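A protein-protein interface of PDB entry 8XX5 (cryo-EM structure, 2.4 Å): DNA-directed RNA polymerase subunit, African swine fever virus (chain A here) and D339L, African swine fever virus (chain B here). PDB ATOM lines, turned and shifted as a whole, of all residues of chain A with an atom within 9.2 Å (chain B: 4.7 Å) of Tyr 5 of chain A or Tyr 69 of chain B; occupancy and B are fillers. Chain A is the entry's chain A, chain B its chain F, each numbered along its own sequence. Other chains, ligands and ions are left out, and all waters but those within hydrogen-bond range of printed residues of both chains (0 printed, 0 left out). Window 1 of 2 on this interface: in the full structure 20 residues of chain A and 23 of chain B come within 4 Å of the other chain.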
ATOM      1  N   GLU A   2      -9.952   0.966   0.617  1.00  0.00           N
ATOM      2  CA  GLU A   2     -11.048   1.798   0.117  1.00  0.00           C
ATOM      3  C   GLU A   2     -12.231   1.792   1.091  1.00  0.00           C
ATOM      4  O   GLU A   2     -13.282   1.202   0.843  1.00  0.00           O
ATOM      5  CB  GLU A   2     -11.482   1.360  -1.287  1.00  0.00           C
ATOM      6  CG  GLU A   2     -12.106   2.478  -2.111  1.00  0.00           C
ATOM      7  CD  GLU A   2     -13.624   2.402  -2.171  1.00  0.00           C
ATOM      8  OE1 GLU A   2     -14.199   1.424  -1.651  1.00  0.00           O
ATOM      9  OE2 GLU A   2     -14.243   3.322  -2.744  1.00  0.00           O
ATOM     10  N   ALA A   3     -12.005   2.429   2.239  1.00  0.00           N
ATOM     11  CA  ALA A   3     -13.077   2.643   3.202  1.00  0.00           C
ATOM     12  C   ALA A   3     -14.228   3.402   2.554  1.00  0.00           C
ATOM     13  O   ALA A   3     -14.085   4.575   2.199  1.00  0.00           O
ATOM     14  CB  ALA A   3     -12.563   3.401   4.426  1.00  0.00           C
ATOM     15  N   GLY A   4     -15.372   2.739   2.396  1.00  0.00           N
ATOM     16  CA  GLY A   4     -16.488   3.350   1.712  1.00  0.00           C
ATOM     17  C   GLY A   4     -17.213   4.372   2.562  1.00  0.00           C
ATOM     18  O   GLY A   4     -17.134   4.375   3.788  1.00  0.00           O
ATOM     19  N   TYR A   5     -17.940   5.253   1.880  1.00  0.00           N
ATOM     20  CA  TYR A   5     -18.694   6.295   2.564  1.00  0.00           C
ATOM     21  C   TYR A   5     -19.785   5.685   3.433  1.00  0.00           C
ATOM     22  O   TYR A   5     -20.452   4.724   3.041  1.00  0.00           O
ATOM     23  CB  TYR A   5     -19.303   7.254   1.544  1.00  0.00           C
ATOM     24  CG  TYR A   5     -20.203   8.310   2.137  1.00  0.00           C
ATOM     25  CD1 TYR A   5     -19.679   9.482   2.658  1.00  0.00           C
ATOM     26  CD2 TYR A   5     -21.578   8.138   2.169  1.00  0.00           C
ATOM     27  CE1 TYR A   5     -20.499  10.450   3.194  1.00  0.00           C
ATOM     28  CE2 TYR A   5     -22.404   9.098   2.703  1.00  0.00           C
ATOM     29  CZ  TYR A   5     -21.861  10.253   3.214  1.00  0.00           C
ATOM     30  OH  TYR A   5     -22.683  11.214   3.748  1.00  0.00           O
ATOM     31  N   ALA A   6     -19.966   6.252   4.621  1.00  0.00           N
ATOM     32  CA  ALA A   6     -20.954   5.752   5.562  1.00  0.00           C
ATOM     33  C   ALA A   6     -21.467   6.903   6.411  1.00  0.00           C
ATOM     34  O   ALA A   6     -20.842   7.963   6.503  1.00  0.00           O
ATOM     35  CB  ALA A   6     -20.375   4.647   6.451  1.00  0.00           C
ATOM     36  N   GLU A   7     -22.623   6.682   7.027  1.00  0.00           N
ATOM     37  CA  GLU A   7     -23.229   7.635   7.945  1.00  0.00           C
ATOM     38  C   GLU A   7     -23.666   6.900   9.201  1.00  0.00           C
ATOM     39  O   GLU A   7     -24.131   5.760   9.130  1.00  0.00           O
ATOM     40  CB  GLU A   7     -24.432   8.343   7.308  1.00  0.00           C
ATOM     41  CG  GLU A   7     -24.066   9.416   6.299  1.00  0.00           C
ATOM     42  CD  GLU A   7     -25.285  10.058   5.667  1.00  0.00           C
ATOM     43  OE1 GLU A   7     -26.280  10.281   6.386  1.00  0.00           O
ATOM     44  OE2 GLU A   7     -25.252  10.339   4.451  1.00  0.00           O
ATOM     45  N   ILE A   8     -23.515   7.553  10.347  1.00  0.00           N
ATOM     46  CA  ILE A   8     -23.925   6.965  11.618  1.00  0.00           C
ATOM     47  C   ILE A   8     -25.439   7.075  11.739  1.00  0.00           C
ATOM     48  O   ILE A   8     -26.001   8.174  11.677  1.00  0.00           O
ATOM     49  CB  ILE A   8     -23.223   7.650  12.800  1.00  0.00           C
ATOM     50  CG1 ILE A   8     -21.728   7.330  12.787  1.00  0.00           C
ATOM     51  CG2 ILE A   8     -23.843   7.210  14.114  1.00  0.00           C
ATOM     52  CD1 ILE A   8     -20.880   8.342  13.517  1.00  0.00           C
ATOM     53  N   SER A1418     -21.715  14.916  12.597  1.00  0.00           N
ATOM     54  CA  SER A1418     -22.407  14.856  11.325  1.00  0.00           C
ATOM     55  C   SER A1418     -23.265  16.104  11.141  1.00  0.00           C
ATOM     56  O   SER A1418     -23.205  17.053  11.924  1.00  0.00           O
ATOM     57  CB  SER A1418     -23.241  13.578  11.246  1.00  0.00           C
ATOM     58  OG  SER A1418     -23.860  13.455   9.978  1.00  0.00           O
ATOM     59  N   VAL A1419     -24.076  16.104  10.090  1.00  0.00           N
ATOM     60  CA  VAL A1419     -24.956  17.227   9.785  1.00  0.00           C
ATOM     61  C   VAL A1419     -26.397  16.752   9.910  1.00  0.00           C
ATOM     62  O   VAL A1419     -26.699  15.602   9.564  1.00  0.00           O
ATOM     63  CB  VAL A1419     -24.678  17.787   8.381  1.00  0.00           C
ATOM     64  CG1 VAL A1419     -24.625  19.306   8.415  1.00  0.00           C
ATOM     65  CG2 VAL A1419     -23.391  17.205   7.825  1.00  0.00           C
ATOM     66  N   ARG A1421     -30.117  15.923   8.932  1.00  0.00           N
ATOM     67  CA  ARG A1421     -30.724  15.567   7.650  1.00  0.00           C
ATOM     68  C   ARG A1421     -32.039  16.329   7.488  1.00  0.00           C
ATOM     69  O   ARG A1421     -33.136  15.772   7.482  1.00  0.00           O
ATOM     70  CB  ARG A1421     -30.927  14.059   7.559  1.00  0.00           C
ATOM     71  CG  ARG A1421     -31.433  13.574   6.208  1.00  0.00           C
ATOM     72  CD  ARG A1421     -31.528  12.061   6.152  1.00  0.00           C
ATOM     73  NE  ARG A1421     -30.410  11.414   6.825  1.00  0.00           N
ATOM     74  CZ  ARG A1421     -29.522  10.638   6.220  1.00  0.00           C
ATOM     75  NH1 ARG A1421     -29.590  10.393   4.923  1.00  0.00           N
ATOM     76  NH2 ARG A1421     -28.542  10.093   6.936  1.00  0.00           N
ATOM     77  N   MET A1425     -30.463  18.919   3.015  1.00  0.00           N
ATOM     78  CA  MET A1425     -30.092  17.518   3.160  1.00  0.00           C
ATOM     79  C   MET A1425     -31.268  16.609   3.472  1.00  0.00           C
ATOM     80  O   MET A1425     -31.065  15.404   3.632  1.00  0.00           O
ATOM     81  CB  MET A1425     -29.033  17.350   4.250  1.00  0.00           C
ATOM     82  CG  MET A1425     -27.905  18.331   4.159  1.00  0.00           C
ATOM     83  SD  MET A1425     -26.794  17.934   2.807  1.00  0.00           S
ATOM     84  CE  MET A1425     -25.474  19.079   3.148  1.00  0.00           C
ATOM     85  N   ASP A1428     -32.290  13.299  -0.518  1.00  0.00           N
ATOM     86  CA  ASP A1428     -31.016  12.931  -1.110  1.00  0.00           C
ATOM     87  C   ASP A1428     -31.101  12.973  -2.630  1.00  0.00           C
ATOM     88  O   ASP A1428     -32.179  12.898  -3.224  1.00  0.00           O
ATOM     89  CB  ASP A1428     -30.583  11.541  -0.654  1.00  0.00           C
ATOM     90  CG  ASP A1428     -31.654  10.511  -0.863  1.00  0.00           C
ATOM     91  OD1 ASP A1428     -32.537  10.382   0.009  1.00  0.00           O
ATOM     92  OD2 ASP A1428     -31.610   9.828  -1.904  1.00  0.00           O
ATOM     93  N   ILE A1429     -29.935  13.092  -3.255  1.00  0.00           N
ATOM     94  CA  ILE A1429     -29.809  13.229  -4.700  1.00  0.00           C
ATOM     95  C   ILE A1429     -29.073  12.012  -5.237  1.00  0.00           C
ATOM     96  O   ILE A1429     -28.046  11.603  -4.683  1.00  0.00           O
ATOM     97  CB  ILE A1429     -29.071  14.524  -5.077  1.00  0.00           C
ATOM     98  CG1 ILE A1429     -29.691  15.719  -4.353  1.00  0.00           C
ATOM     99  CG2 ILE A1429     -29.095  14.731  -6.577  1.00  0.00           C
ATOM    100  CD1 ILE A1429     -31.117  16.002  -4.749  1.00  0.00           C
ATOM    101  N   ILE A1430     -29.605  11.429  -6.308  1.00  0.00           N
ATOM    102  CA  ILE A1430     -28.953  10.340  -7.016  1.00  0.00           C
ATOM    103  C   ILE A1430     -28.768  10.765  -8.467  1.00  0.00           C
ATOM    104  O   ILE A1430     -29.418  11.691  -8.956  1.00  0.00           O
ATOM    105  CB  ILE A1430     -29.745   9.020  -6.925  1.00  0.00           C
ATOM    106  CG1 ILE A1430     -30.923   9.031  -7.898  1.00  0.00           C
ATOM    107  CG2 ILE A1430     -30.234   8.790  -5.510  1.00  0.00           C
ATOM    108  CD1 ILE A1430     -31.954   7.963  -7.624  1.00  0.00           C
ATOM    109  N   MET A1431     -27.857  10.083  -9.152  1.00  0.00           N
ATOM    110  CA  MET A1431     -27.571  10.375 -10.548  1.00  0.00           C
ATOM    111  C   MET A1431     -28.585   9.670 -11.441  1.00  0.00           C
ATOM    112  O   MET A1431     -28.881   8.489 -11.243  1.00  0.00           O
ATOM    113  CB  MET A1431     -26.151   9.940 -10.911  1.00  0.00           C
ATOM    114  CG  MET A1431     -25.095  10.386  -9.917  1.00  0.00           C
ATOM    115  SD  MET A1431     -24.696  12.140 -10.012  1.00  0.00           S
ATOM    116  CE  MET A1431     -24.565  12.387 -11.777  1.00  0.00           C
ATOM    117  N   GLU A1433     -28.998   7.774 -14.108  1.00  0.00           N
ATOM    118  CA  GLU A1433     -28.094   6.967 -14.923  1.00  0.00           C
ATOM    119  C   GLU A1433     -28.588   6.849 -16.359  1.00  0.00           C
ATOM    120  O   GLU A1433     -27.800   6.986 -17.301  1.00  0.00           O
ATOM    121  CB  GLU A1433     -27.921   5.585 -14.298  1.00  0.00           C
ATOM    122  CG  GLU A1433     -26.773   5.502 -13.310  1.00  0.00           C
ATOM    123  CD  GLU A1433     -27.127   4.714 -12.066  1.00  0.00           C
ATOM    124  OE1 GLU A1433     -28.275   4.231 -11.972  1.00  0.00           O
ATOM    125  OE2 GLU A1433     -26.256   4.576 -11.182  1.00  0.00           O
ATOM    126  N   THR B  10     -19.391  -0.662  -0.100  1.00  0.00           N
ATOM    127  CA  THR B  10     -19.732   0.672  -0.574  1.00  0.00           C
ATOM    128  C   THR B  10     -18.505   1.251  -1.255  1.00  0.00           C
ATOM    129  O   THR B  10     -17.444   1.367  -0.635  1.00  0.00           O
ATOM    130  CB  THR B  10     -20.184   1.576   0.575  1.00  0.00           C
ATOM    131  OG1 THR B  10     -21.415   1.086   1.115  1.00  0.00           O
ATOM    132  CG2 THR B  10     -20.385   2.999   0.085  1.00  0.00           C
ATOM    133  N   LEU B  11     -18.644   1.597  -2.527  1.00  0.00           N
ATOM    134  CA  LEU B  11     -17.557   2.227  -3.253  1.00  0.00           C
ATOM    135  C   LEU B  11     -17.574   3.732  -3.018  1.00  0.00           C
ATOM    136  O   LEU B  11     -18.466   4.276  -2.368  1.00  0.00           O
ATOM    137  CB  LEU B  11     -17.654   1.909  -4.745  1.00  0.00           C
ATOM    138  CG  LEU B  11     -17.462   0.438  -5.115  1.00  0.00           C
ATOM    139  CD1 LEU B  11     -17.108   0.302  -6.581  1.00  0.00           C
ATOM    140  CD2 LEU B  11     -16.393  -0.208  -4.244  1.00  0.00           C
ATOM    141  N   ASN B  12     -16.548   4.405  -3.521  1.00  0.00           N
ATOM    142  CA  ASN B  12     -16.491   5.858  -3.530  1.00  0.00           C
ATOM    143  C   ASN B  12     -16.278   6.310  -4.964  1.00  0.00           C
ATOM    144  O   ASN B  12     -15.395   5.794  -5.656  1.00  0.00           O
ATOM    145  CB  ASN B  12     -15.377   6.385  -2.624  1.00  0.00           C
ATOM    146  CG  ASN B  12     -15.730   6.291  -1.155  1.00  0.00           C
ATOM    147  OD1 ASN B  12     -16.901   6.223  -0.790  1.00  0.00           O
ATOM    148  ND2 ASN B  12     -14.715   6.291  -0.302  1.00  0.00           N
ATOM    149  N   ILE B  13     -17.092   7.256  -5.409  1.00  0.00           N
ATOM    150  CA  ILE B  13     -17.094   7.702  -6.793  1.00  0.00           C
ATOM    151  C   ILE B  13     -16.702   9.172  -6.813  1.00  0.00           C
ATOM    152  O   ILE B  13     -17.482  10.037  -6.399  1.00  0.00           O
ATOM    153  CB  ILE B  13     -18.459   7.481  -7.452  1.00  0.00           C
ATOM    154  CG1 ILE B  13     -18.792   5.989  -7.492  1.00  0.00           C
ATOM    155  CG2 ILE B  13     -18.452   8.052  -8.833  1.00  0.00           C
ATOM    156  CD1 ILE B  13     -20.243   5.689  -7.262  1.00  0.00           C
ATOM    157  N   PHE B  58     -25.825   7.443  -5.020  1.00  0.00           N
ATOM    158  CA  PHE B  58     -26.177   8.515  -4.101  1.00  0.00           C
ATOM    159  C   PHE B  58     -25.042   9.524  -4.012  1.00  0.00           C
ATOM    160  O   PHE B  58     -23.868   9.154  -3.997  1.00  0.00           O
ATOM    161  CB  PHE B  58     -26.464   7.967  -2.706  1.00  0.00           C
ATOM    162  CG  PHE B  58     -27.439   6.834  -2.676  1.00  0.00           C
ATOM    163  CD1 PHE B  58     -28.790   7.062  -2.832  1.00  0.00           C
ATOM    164  CD2 PHE B  58     -27.005   5.542  -2.453  1.00  0.00           C
ATOM    165  CE1 PHE B  58     -29.687   6.019  -2.795  1.00  0.00           C
ATOM    166  CE2 PHE B  58     -27.898   4.498  -2.412  1.00  0.00           C
ATOM    167  CZ  PHE B  58     -29.241   4.735  -2.583  1.00  0.00           C
ATOM    168  N   ILE B  59     -25.395  10.797  -3.932  1.00  0.00           N
ATOM    169  CA  ILE B  59     -24.409  11.852  -3.737  1.00  0.00           C
ATOM    170  C   ILE B  59     -24.088  11.960  -2.255  1.00  0.00           C
ATOM    171  O   ILE B  59     -24.981  11.861  -1.405  1.00  0.00           O
ATOM    172  CB  ILE B  59     -24.927  13.186  -4.306  1.00  0.00           C
ATOM    173  CG1 ILE B  59     -25.187  13.054  -5.805  1.00  0.00           C
ATOM    174  CG2 ILE B  59     -23.933  14.307  -4.046  1.00  0.00           C
ATOM    175  CD1 ILE B  59     -24.052  12.405  -6.554  1.00  0.00           C
ATOM    176  N   MET B  60     -22.807  12.145  -1.936  1.00  0.00           N
ATOM    177  CA  MET B  60     -22.402  12.277  -0.542  1.00  0.00           C
ATOM    178  C   MET B  60     -23.102  13.461   0.106  1.00  0.00           C
ATOM    179  O   MET B  60     -23.145  14.560  -0.452  1.00  0.00           O
ATOM    180  CB  MET B  60     -20.887  12.439  -0.432  1.00  0.00           C
ATOM    181  CG  MET B  60     -20.133  11.132  -0.328  1.00  0.00           C
ATOM    182  SD  MET B  60     -18.458  11.230  -0.968  1.00  0.00           S
ATOM    183  CE  MET B  60     -18.183   9.529  -1.444  1.00  0.00           C
ATOM    184  N   ARG B  61     -23.645  13.229   1.297  1.00  0.00           N
ATOM    185  CA  ARG B  61     -24.477  14.205   1.981  1.00  0.00           C
ATOM    186  C   ARG B  61     -23.735  14.995   3.049  1.00  0.00           C
ATOM    187  O   ARG B  61     -24.074  16.156   3.288  1.00  0.00           O
ATOM    188  CB  ARG B  61     -25.680  13.502   2.619  1.00  0.00           C
ATOM    189  CG  ARG B  61     -26.810  14.419   3.016  1.00  0.00           C
ATOM    190  CD  ARG B  61     -27.951  13.640   3.649  1.00  0.00           C
ATOM    191  NE  ARG B  61     -27.568  13.008   4.906  1.00  0.00           N
ATOM    192  CZ  ARG B  61     -27.273  13.656   6.025  1.00  0.00           C
ATOM    193  NH1 ARG B  61     -27.314  14.976   6.093  1.00  0.00           N
ATOM    194  NH2 ARG B  61     -26.929  12.961   7.105  1.00  0.00           N
ATOM    195  N   THR B  62     -22.727  14.406   3.685  1.00  0.00           N
ATOM    196  CA  THR B  62     -22.078  15.016   4.836  1.00  0.00           C
ATOM    197  C   THR B  62     -20.857  15.849   4.473  1.00  0.00           C
ATOM    198  O   THR B  62     -20.180  16.350   5.374  1.00  0.00           O
ATOM    199  CB  THR B  62     -21.677  13.937   5.844  1.00  0.00           C
ATOM    200  OG1 THR B  62     -20.936  12.910   5.176  1.00  0.00           O
ATOM    201  CG2 THR B  62     -22.913  13.323   6.475  1.00  0.00           C
ATOM    202  N   ASN B  63     -20.558  16.011   3.187  1.00  0.00           N
ATOM    203  CA  ASN B  63     -19.467  16.869   2.753  1.00  0.00           C
ATOM    204  C   ASN B  63     -19.906  17.637   1.515  1.00  0.00           C
ATOM    205  O   ASN B  63     -20.936  17.340   0.906  1.00  0.00           O
ATOM    206  CB  ASN B  63     -18.186  16.068   2.480  1.00  0.00           C
ATOM    207  CG  ASN B  63     -18.433  14.846   1.624  1.00  0.00           C
ATOM    208  OD1 ASN B  63     -18.341  14.904   0.400  1.00  0.00           O
ATOM    209  ND2 ASN B  63     -18.746  13.727   2.265  1.00  0.00           N
ATOM    210  N   ARG B  67     -19.217  14.141  -4.485  1.00  0.00           N
ATOM    211  CA  ARG B  67     -18.909  12.776  -4.872  1.00  0.00           C
ATOM    212  C   ARG B  67     -20.065  11.841  -4.530  1.00  0.00           C
ATOM    213  O   ARG B  67     -20.915  12.137  -3.687  1.00  0.00           O
ATOM    214  CB  ARG B  67     -17.632  12.304  -4.182  1.00  0.00           C
ATOM    215  CG  ARG B  67     -16.368  12.954  -4.703  1.00  0.00           C
ATOM    216  CD  ARG B  67     -15.339  13.119  -3.602  1.00  0.00           C
ATOM    217  NE  ARG B  67     -15.081  11.867  -2.901  1.00  0.00           N
ATOM    218  CZ  ARG B  67     -15.056  11.739  -1.582  1.00  0.00           C
ATOM    219  NH1 ARG B  67     -15.271  12.771  -0.783  1.00  0.00           N
ATOM    220  NH2 ARG B  67     -14.810  10.545  -1.051  1.00  0.00           N
ATOM    221  N   GLY B  68     -20.091  10.698  -5.209  1.00  0.00           N
ATOM    222  CA  GLY B  68     -21.074   9.672  -4.933  1.00  0.00           C
ATOM    223  C   GLY B  68     -20.436   8.447  -4.317  1.00  0.00           C
ATOM    224  O   GLY B  68     -19.210   8.320  -4.355  1.00  0.00           O
ATOM    225  N   TYR B  69     -21.222   7.547  -3.727  1.00  0.00           N
ATOM    226  CA  TYR B  69     -20.636   6.342  -3.152  1.00  0.00           C
ATOM    227  C   TYR B  69     -21.155   5.060  -3.790  1.00  0.00           C
ATOM    228  O   TYR B  69     -20.345   4.267  -4.278  1.00  0.00           O
ATOM    229  CB  TYR B  69     -20.822   6.304  -1.626  1.00  0.00           C
ATOM    230  CG  TYR B  69     -22.169   6.712  -1.074  1.00  0.00           C
ATOM    231  CD1 TYR B  69     -22.557   8.045  -1.031  1.00  0.00           C
ATOM    232  CD2 TYR B  69     -23.032   5.764  -0.543  1.00  0.00           C
ATOM    233  CE1 TYR B  69     -23.774   8.414  -0.505  1.00  0.00           C
ATOM    234  CE2 TYR B  69     -24.249   6.125  -0.016  1.00  0.00           C
ATOM    235  CZ  TYR B  69     -24.615   7.450   0.004  1.00  0.00           C
ATOM    236  OH  TYR B  69     -25.832   7.809   0.529  1.00  0.00           O
ATOM    237  N   MET B  70     -22.470   4.827  -3.805  1.00  0.00           N
ATOM    238  CA  MET B  70     -23.068   3.600  -4.336  1.00  0.00           C
ATOM    239  C   MET B  70     -22.706   2.362  -3.516  1.00  0.00           C
ATOM    240  O   MET B  70     -21.543   2.154  -3.162  1.00  0.00           O
ATOM    241  CB  MET B  70     -22.673   3.384  -5.803  1.00  0.00           C
ATOM    242  CG  MET B  70     -23.066   2.024  -6.359  1.00  0.00           C
ATOM    243  SD  MET B  70     -22.919   1.897  -8.150  1.00  0.00           S
ATOM    244  CE  MET B  70     -23.854   3.327  -8.677  1.00  0.00           C
ATOM    245  N   HIS B  71     -23.700   1.531  -3.216  1.00  0.00           N
ATOM    246  CA  HIS B  71     -23.487   0.249  -2.559  1.00  0.00           C
ATOM    247  C   HIS B  71     -23.499  -0.863  -3.597  1.00  0.00           C
ATOM    248  O   HIS B  71     -24.349  -0.881  -4.491  1.00  0.00           O
ATOM    249  CB  HIS B  71     -24.560  -0.015  -1.501  1.00  0.00           C
ATOM    250  CG  HIS B  71     -24.725   1.099  -0.517  1.00  0.00           C
ATOM    251  ND1 HIS B  71     -23.682   1.586   0.239  1.00  0.00           N
ATOM    252  CD2 HIS B  71     -25.814   1.820  -0.163  1.00  0.00           C
ATOM    253  CE1 HIS B  71     -24.120   2.560   1.017  1.00  0.00           C
ATOM    254  NE2 HIS B  71     -25.411   2.721   0.791  1.00  0.00           N
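N of Asn 12 of chain B lies within hydrogen-bond range of OE2 of Glu 2 of chain A, at 2.7 Å.
ND2 of Asn 12 of chain B sits at hydrogen-bond distance from O of Ala 3 of chain A, 3.1 Å away.
N of Tyr 5 of chain A sits at hydrogen-bond distance from OD1 of Asn 12 of chain B (3.0 Å).
The backbone carbonyl oxygen of Ile 1429 of chain A lies within hydrogen-bond range of the backbone NH of Ile 59 of chain B, 2.9 Å away.
The side-chain hydroxyl (OH) of Tyr 5 of chain A is in hydrogen-bond range of the backbone NH (N) of Arg 61 of chain B (3.3 Å).
The side-chain carboxylate (OE1) of Glu 7 of chain A is in salt-bridge range of the guanidinium group (NH2) of Arg 61 of chain B.
OG1 of Thr 62 of chain B sits at hydrogen-bond distance from OH of Tyr 5 of chain A (2.8 Å).
The side-chain carboxylate (OE1) of Glu 2 of chain A lies close to the backbone carbonyl oxygen (O) of Thr 10 of chain B (3.4 Å).
NH2 of Arg 1421 of chain A sits close to NH2 of Arg 61 of chain B, at 3.3 Å.
The side-chain sulfur (SD) of Met 1425 of chain A lies close to the backbone carbonyl oxygen (O) of Arg 61 of chain B.
The backbone carbonyl oxygen (O) of Leu 11 of chain B sits close to the backbone carbonyl oxygen (O) of Tyr 69 of chain B (2.7 Å).
The backbone NH (N) of Leu 11 of chain B is in hydrogen-bond range of the backbone carbonyl oxygen (O) of Met 70 of chain B.
The backbone carbonyl oxygen of Phe 58 of chain B sits at hydrogen-bond distance from the backbone NH of Tyr 69 of chain B (3.1 Å).
N of Met 60 of chain B sits at hydrogen-bond distance from O of Arg 67 of chain B (2.6 Å).
The side-chain hydroxyl (OH) of Tyr 5 of chain A sits at hydrogen-bond distance from the side-chain carboxylate (OE2) of Glu 7 of chain A (2.8 Å).
NH1 of Arg 1421 of chain A lies within salt-bridge range of OE1 of Glu 7 of chain A (3.6 Å).
Among the printed residues, pairs that only touch across the chains: Gly 4 of chain A with Thr 10 of chain B (3.2 Å), Tyr 5 of chain A with Tyr 69 of chain B (3.3 Å), Glu 2 of chain A with Leu 11 of chain B (3.4 Å), Tyr 5 of chain A with Thr 10 of chain B (3.4 Å), Tyr 5 of chain A with Met 60 of chain B (3.4 Å), Ile 1430 of chain A with Phe 58 of chain B (3.5 Å), Met 1431 of chain A with Ile 59 of chain B (3.5 Å), Val 1419 of chain A with Arg 61 of chain B (3.6 Å), Ser 1418 of chain A with Thr 62 of chain B (3.6 Å), Ile 1429 of chain A with Phe 58 of chain B (3.7 Å), Glu 1433 of chain A with Met 70 of chain B (3.7 Å), Tyr 5 of chain A with Asn 63 of chain B (3.8 Å), Gly 4 of chain A with Asn 12 of chain B (3.8 Å) and Val 1419 of chain A with Thr 62 of chain B (3.9 Å).
Of chain B, only Thr 10, Asn 12, Met 60, Arg 61, Thr 62, Asn 63 and Tyr 69 come within 4 Å of Tyr 5 of chain A.
Of the printed residues of chain A, Tyr 69 of chain B touches Tyr 5.
Of the printed residues of chain A, Met 70 of chain B touches Glu 1433.
Printed residues of chain B within 4 Å of Glu 2 of chain A: Thr 10, Leu 11 and Asn 12.
Of the printed residues of chain A, Leu 11 of chain B touches Glu 2.
Printed residues of chain B within 4 Å of Ile 1429 of chain A: Phe 58 and Ile 59.
Of the printed residues of chain B, Met 1431 of chain A touches Ile 59.
Ala 6 of chain A touches none of the printed residues of chain B.
Ile 13 of chain B touches none of the printed residues of chain A.
The nearest residue of chain B that does not touch Tyr 5 of chain A is Leu 11 of chain B (4.4 Å).
Of the 16 printed residues of chain A, 13 touch a printed residue of chain B.
Printed residues of chain A that touch a printed residue of chain B: Glu 2, Ala 3, Gly 4, Tyr 5, Glu 7, Ser 1418, Val 1419, Arg 1421, Met 1425, Ile 1429, Ile 1430, Met 1431 and Glu 1433.
Of the 15 printed residues of chain B, 11 touch a printed residue of chain A.
Printed residues of chain B that touch a printed residue of chain A: Thr 10, Leu 11, Asn 12, Phe 58, Ile 59, Met 60, Arg 61, Thr 62, Asn 63, Tyr 69 and Met 70.
Hydrophobic or aromatic side chains of chain B that line the printed part of chain A: Leu 11, Phe 58, Ile 59, Met 60, Tyr 69 and Met 70.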
